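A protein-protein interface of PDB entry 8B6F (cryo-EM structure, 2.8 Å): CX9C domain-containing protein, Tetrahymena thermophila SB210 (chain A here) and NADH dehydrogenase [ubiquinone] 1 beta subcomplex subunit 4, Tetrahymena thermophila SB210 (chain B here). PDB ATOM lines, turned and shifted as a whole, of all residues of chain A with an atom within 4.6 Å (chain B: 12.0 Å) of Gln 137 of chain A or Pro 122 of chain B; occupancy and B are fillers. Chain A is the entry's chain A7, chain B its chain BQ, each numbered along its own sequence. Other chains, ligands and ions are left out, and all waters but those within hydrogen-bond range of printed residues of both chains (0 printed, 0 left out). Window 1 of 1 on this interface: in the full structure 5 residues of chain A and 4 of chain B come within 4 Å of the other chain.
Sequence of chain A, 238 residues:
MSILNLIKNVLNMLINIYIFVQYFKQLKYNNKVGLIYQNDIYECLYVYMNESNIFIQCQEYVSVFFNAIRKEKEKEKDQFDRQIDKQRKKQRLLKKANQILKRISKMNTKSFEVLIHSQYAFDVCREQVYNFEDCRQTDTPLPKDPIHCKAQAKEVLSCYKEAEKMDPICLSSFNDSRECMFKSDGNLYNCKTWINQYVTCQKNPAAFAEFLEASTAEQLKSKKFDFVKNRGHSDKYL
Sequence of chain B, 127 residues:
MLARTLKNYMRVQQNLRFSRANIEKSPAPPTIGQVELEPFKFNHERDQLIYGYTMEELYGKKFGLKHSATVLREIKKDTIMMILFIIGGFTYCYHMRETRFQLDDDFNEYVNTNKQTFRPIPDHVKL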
ATOM      1  N   GLU A 133      22.664 -17.767  33.856  1.00  0.00           N
ATOM      2  CA  GLU A 133      22.921 -17.133  32.566  1.00  0.00           C
ATOM      3  C   GLU A 133      21.795 -17.415  31.580  1.00  0.00           C
ATOM      4  O   GLU A 133      21.320 -16.509  30.888  1.00  0.00           O
ATOM      5  CB  GLU A 133      24.261 -17.604  32.008  1.00  0.00           C
ATOM      6  CG  GLU A 133      25.453 -17.076  32.785  1.00  0.00           C
ATOM      7  CD  GLU A 133      26.772 -17.577  32.239  1.00  0.00           C
ATOM      8  OE1 GLU A 133      26.765 -18.237  31.180  1.00  0.00           O
ATOM      9  OE2 GLU A 133      27.817 -17.313  32.869  1.00  0.00           O
ATOM     10  N   ASP A 134      21.349 -18.670  31.506  1.00  0.00           N
ATOM     11  CA  ASP A 134      20.250 -19.016  30.610  1.00  0.00           C
ATOM     12  C   ASP A 134      18.980 -18.260  30.972  1.00  0.00           C
ATOM     13  O   ASP A 134      18.257 -17.787  30.089  1.00  0.00           O
ATOM     14  CB  ASP A 134      19.993 -20.521  30.649  1.00  0.00           C
ATOM     15  CG  ASP A 134      21.040 -21.312  29.903  1.00  0.00           C
ATOM     16  OD1 ASP A 134      22.221 -21.265  30.303  1.00  0.00           O
ATOM     17  OD2 ASP A 134      20.684 -21.983  28.914  1.00  0.00           O
ATOM     18  N   CYS A 135      18.690 -18.136  32.266  1.00  0.00           N
ATOM     19  CA  CYS A 135      17.500 -17.409  32.689  1.00  0.00           C
ATOM     20  C   CYS A 135      17.569 -15.942  32.278  1.00  0.00           C
ATOM     21  O   CYS A 135      16.568 -15.367  31.835  1.00  0.00           O
ATOM     22  CB  CYS A 135      17.321 -17.546  34.200  1.00  0.00           C
ATOM     23  SG  CYS A 135      15.717 -16.999  34.803  1.00  0.00           S
ATOM     24  N   ARG A 136      18.739 -15.317  32.417  1.00  0.00           N
ATOM     25  CA  ARG A 136      18.879 -13.895  32.120  1.00  0.00           C
ATOM     26  C   ARG A 136      19.087 -13.601  30.639  1.00  0.00           C
ATOM     27  O   ARG A 136      19.088 -12.426  30.259  1.00  0.00           O
ATOM     28  CB  ARG A 136      20.048 -13.303  32.914  1.00  0.00           C
ATOM     29  CG  ARG A 136      21.396 -13.898  32.553  1.00  0.00           C
ATOM     30  CD  ARG A 136      22.534 -13.273  33.341  1.00  0.00           C
ATOM     31  NE  ARG A 136      22.886 -11.955  32.826  1.00  0.00           N
ATOM     32  CZ  ARG A 136      22.381 -10.810  33.264  1.00  0.00           C
ATOM     33  NH1 ARG A 136      21.489 -10.773  34.241  1.00  0.00           N
ATOM     34  NH2 ARG A 136      22.779  -9.671  32.705  1.00  0.00           N
ATOM     35  N   GLN A 137      19.267 -14.618  29.799  1.00  0.00           N
ATOM     36  CA  GLN A 137      19.483 -14.380  28.377  1.00  0.00           C
ATOM     37  C   GLN A 137      18.313 -13.612  27.772  1.00  0.00           C
ATOM     38  O   GLN A 137      17.151 -13.836  28.121  1.00  0.00           O
ATOM     39  CB  GLN A 137      19.676 -15.707  27.643  1.00  0.00           C
ATOM     40  CG  GLN A 137      21.099 -16.250  27.690  1.00  0.00           C
ATOM     41  CD  GLN A 137      22.058 -15.464  26.824  1.00  0.00           C
ATOM     42  OE1 GLN A 137      21.726 -14.391  26.323  1.00  0.00           O
ATOM     43  NE2 GLN A 137      23.257 -16.001  26.633  1.00  0.00           N
ATOM     44  N   THR A 138      18.629 -12.700  26.853  1.00  0.00           N
ATOM     45  CA  THR A 138      17.637 -11.854  26.207  1.00  0.00           C
ATOM     46  C   THR A 138      18.061 -11.619  24.764  1.00  0.00           C
ATOM     47  O   THR A 138      19.214 -11.843  24.391  1.00  0.00           O
ATOM     48  CB  THR A 138      17.478 -10.514  26.948  1.00  0.00           C
ATOM     49  OG1 THR A 138      17.348 -10.756  28.352  1.00  0.00           O
ATOM     50  CG2 THR A 138      16.249  -9.756  26.472  1.00  0.00           C
ATOM     51  N   LYS A 144      17.578  -8.018  31.455  1.00  0.00           N
ATOM     52  CA  LYS A 144      16.293  -8.613  31.777  1.00  0.00           C
ATOM     53  C   LYS A 144      15.915  -8.288  33.219  1.00  0.00           C
ATOM     54  O   LYS A 144      16.766  -8.000  34.062  1.00  0.00           O
ATOM     55  CB  LYS A 144      16.343 -10.126  31.569  1.00  0.00           C
ATOM     56  CG  LYS A 144      14.992 -10.816  31.586  1.00  0.00           C
ATOM     57  CD  LYS A 144      15.132 -12.284  31.215  1.00  0.00           C
ATOM     58  CE  LYS A 144      13.782 -12.972  31.156  1.00  0.00           C
ATOM     59  NZ  LYS A 144      13.909 -14.398  30.743  1.00  0.00           N
ATOM     60  N   THR B 117      34.263 -24.011  24.689  1.00  0.00           N
ATOM     61  CA  THR B 117      32.854 -24.316  24.901  1.00  0.00           C
ATOM     62  C   THR B 117      31.988 -23.169  24.403  1.00  0.00           C
ATOM     63  O   THR B 117      32.217 -22.009  24.760  1.00  0.00           O
ATOM     64  CB  THR B 117      32.567 -24.583  26.379  1.00  0.00           C
ATOM     65  OG1 THR B 117      33.170 -23.562  27.184  1.00  0.00           O
ATOM     66  CG2 THR B 117      33.101 -25.945  26.783  1.00  0.00           C
ATOM     67  N   PHE B 118      30.997 -23.499  23.581  1.00  0.00           N
ATOM     68  CA  PHE B 118      30.019 -22.542  23.082  1.00  0.00           C
ATOM     69  C   PHE B 118      28.647 -22.966  23.583  1.00  0.00           C
ATOM     70  O   PHE B 118      28.215 -24.096  23.333  1.00  0.00           O
ATOM     71  CB  PHE B 118      30.043 -22.476  21.553  1.00  0.00           C
ATOM     72  CG  PHE B 118      31.393 -22.153  20.982  1.00  0.00           C
ATOM     73  CD1 PHE B 118      32.352 -23.143  20.838  1.00  0.00           C
ATOM     74  CD2 PHE B 118      31.700 -20.865  20.580  1.00  0.00           C
ATOM     75  CE1 PHE B 118      33.594 -22.850  20.313  1.00  0.00           C
ATOM     76  CE2 PHE B 118      32.939 -20.565  20.054  1.00  0.00           C
ATOM     77  CZ  PHE B 118      33.887 -21.559  19.919  1.00  0.00           C
ATOM     78  N   ARG B 119      27.968 -22.063  24.290  1.00  0.00           N
ATOM     79  CA  ARG B 119      26.655 -22.355  24.842  1.00  0.00           C
ATOM     80  C   ARG B 119      25.580 -21.774  23.937  1.00  0.00           C
ATOM     81  O   ARG B 119      25.549 -20.548  23.749  1.00  0.00           O
ATOM     82  CB  ARG B 119      26.525 -21.784  26.246  1.00  0.00           C
ATOM     83  CG  ARG B 119      27.362 -22.519  27.282  1.00  0.00           C
ATOM     84  CD  ARG B 119      27.019 -22.076  28.692  1.00  0.00           C
ATOM     85  NE  ARG B 119      25.599 -22.241  28.984  1.00  0.00           N
ATOM     86  CZ  ARG B 119      25.021 -23.398  29.271  1.00  0.00           C
ATOM     87  NH1 ARG B 119      25.710 -24.527  29.305  1.00  0.00           N
ATOM     88  NH2 ARG B 119      23.716 -23.425  29.527  1.00  0.00           N
ATOM     89  N   PRO B 120      24.689 -22.584  23.366  1.00  0.00           N
ATOM     90  CA  PRO B 120      23.653 -22.025  22.490  1.00  0.00           C
ATOM     91  C   PRO B 120      22.689 -21.134  23.254  1.00  0.00           C
ATOM     92  O   PRO B 120      22.450 -21.315  24.449  1.00  0.00           O
ATOM     93  CB  PRO B 120      22.945 -23.269  21.942  1.00  0.00           C
ATOM     94  CG  PRO B 120      23.169 -24.310  22.974  1.00  0.00           C
ATOM     95  CD  PRO B 120      24.527 -24.037  23.546  1.00  0.00           C
ATOM     96  N   ILE B 121      22.136 -20.160  22.543  1.00  0.00           N
ATOM     97  CA  ILE B 121      21.172 -19.242  23.162  1.00  0.00           C
ATOM     98  C   ILE B 121      19.912 -20.017  23.526  1.00  0.00           C
ATOM     99  O   ILE B 121      19.506 -20.919  22.771  1.00  0.00           O
ATOM    100  CB  ILE B 121      20.857 -18.084  22.212  1.00  0.00           C
ATOM    101  CG1 ILE B 121      22.145 -17.342  21.836  1.00  0.00           C
ATOM    102  CG2 ILE B 121      19.863 -17.126  22.858  1.00  0.00           C
ATOM    103  CD1 ILE B 121      21.954 -16.221  20.832  1.00  0.00           C
ATOM    104  N   PRO B 122      19.260 -19.721  24.652  1.00  0.00           N
ATOM    105  CA  PRO B 122      18.040 -20.457  25.004  1.00  0.00           C
ATOM    106  C   PRO B 122      16.938 -20.249  23.977  1.00  0.00           C
ATOM    107  O   PRO B 122      16.852 -19.209  23.322  1.00  0.00           O
ATOM    108  CB  PRO B 122      17.652 -19.873  26.367  1.00  0.00           C
ATOM    109  CG  PRO B 122      18.910 -19.317  26.913  1.00  0.00           C
ATOM    110  CD  PRO B 122      19.671 -18.809  25.731  1.00  0.00           C
ATOM    111  N   ASP B 123      16.082 -21.264  23.845  1.00  0.00           N
ATOM    112  CA  ASP B 123      14.989 -21.206  22.882  1.00  0.00           C
ATOM    113  C   ASP B 123      13.955 -20.146  23.234  1.00  0.00           C
ATOM    114  O   ASP B 123      13.203 -19.721  22.352  1.00  0.00           O
ATOM    115  CB  ASP B 123      14.306 -22.570  22.782  1.00  0.00           C
ATOM    116  CG  ASP B 123      15.268 -23.674  22.396  1.00  0.00           C
ATOM    117  OD1 ASP B 123      16.251 -23.384  21.685  1.00  0.00           O
ATOM    118  OD2 ASP B 123      15.041 -24.832  22.805  1.00  0.00           O
ATOM    119  N   HIS B 124      13.892 -19.719  24.494  1.00  0.00           N
ATOM    120  CA  HIS B 124      12.912 -18.724  24.908  1.00  0.00           C
ATOM    121  C   HIS B 124      13.269 -17.312  24.465  1.00  0.00           C
ATOM    122  O   HIS B 124      12.428 -16.415  24.585  1.00  0.00           O
ATOM    123  CB  HIS B 124      12.744 -18.755  26.430  1.00  0.00           C
ATOM    124  CG  HIS B 124      13.977 -18.368  27.185  1.00  0.00           C
ATOM    125  ND1 HIS B 124      14.466 -17.079  27.204  1.00  0.00           N
ATOM    126  CD2 HIS B 124      14.818 -19.099  27.953  1.00  0.00           C
ATOM    127  CE1 HIS B 124      15.557 -17.035  27.948  1.00  0.00           C
ATOM    128  NE2 HIS B 124      15.792 -18.247  28.416  1.00  0.00           N
ATOM    129  N   VAL B 125      14.484 -17.087  23.963  1.00  0.00           N
ATOM    130  CA  VAL B 125      14.888 -15.741  23.566  1.00  0.00           C
ATOM    131  C   VAL B 125      14.118 -15.301  22.326  1.00  0.00           C
ATOM    132  O   VAL B 125      13.382 -14.309  22.351  1.00  0.00           O
ATOM    133  CB  VAL B 125      16.408 -15.683  23.336  1.00  0.00           C
ATOM    134  CG1 VAL B 125      16.817 -14.351  22.721  1.00  0.00           C
ATOM    135  CG2 VAL B 125      17.144 -15.909  24.646  1.00  0.00           C
ATOM    136  N   LYS B 126      14.274 -16.034  21.230  1.00  0.00           N
ATOM    137  CA  LYS B 126      13.600 -15.698  19.982  1.00  0.00           C
ATOM    138  C   LYS B 126      13.900 -14.262  19.567  1.00  0.00           C
ATOM    139  O   LYS B 126      13.249 -13.715  18.677  1.00  0.00           O
ATOM    140  CB  LYS B 126      12.089 -15.900  20.115  1.00  0.00           C
ATOM    141  CG  LYS B 126      11.687 -17.341  20.374  1.00  0.00           C
ATOM    142  CD  LYS B 126      10.180 -17.483  20.507  1.00  0.00           C
ATOM    143  CE  LYS B 126       9.776 -18.938  20.691  1.00  0.00           C
ATOM    144  NZ  LYS B 126      10.401 -19.549  21.898  1.00  0.00           N
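Among the printed residues, pairs that only touch across the chains: Gln 137 of chain A with Pro 122 of chain B (3.5 Å), Gln 137 of chain A with His 124 of chain B (3.6 Å), Asp 134 of chain A with Pro 122 of chain B (3.6 Å), Thr 138 of chain A with Val 125 of chain B (3.6 Å) and Gln 137 of chain A with Val 125 of chain B (3.9 Å).
The side-chain hydroxyl of Thr 138 of chain A is in hydrogen-bond range of the backbone carbonyl oxygen of Arg 136 of chain A (3.1 Å).
Gln 137 of chain A touches just these residues of chain B: Pro 122, His 124 and Val 125. Of the printed residues of chain A, Pro 122 of chain B touches Asp 134 and Gln 137. No residue of chain B comes within 4 Å of Glu 133 of chain A. Of chain B, only Arg 119 (2.7 Å), Pro 122 (3.6 Å) and His 124 (3.0 Å) come within 4 Å of Asp 134 of chain A. No residue of chain B comes within 4 Å of Cys 135 of chain A. No residue of chain B comes within 4 Å of Arg 136 of chain A. Thr 138 of chain A touches just one residue of chain B: Val 125. Printed residues of chain A within 4 Å of Arg 119 of chain B: Asp 134 (2.7 Å). Of the printed residues of chain A, Val 125 of chain B touches Gln 137 (3.9 Å) and Thr 138 (3.6 Å).
Printed residues of chain A that touch a printed residue of chain B: Asp 134, Gln 137 and Thr 138.
The backbone carbonyl oxygen of Asp 134 of chain A is in hydrogen-bond range of a ring nitrogen (NE2) of His 124 of chain B. The side-chain carboxylate (OD1) of Asp 134 of chain A is in salt-bridge range of the guanidinium group (NH2) of Arg 119 of chain B (2.7 Å).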
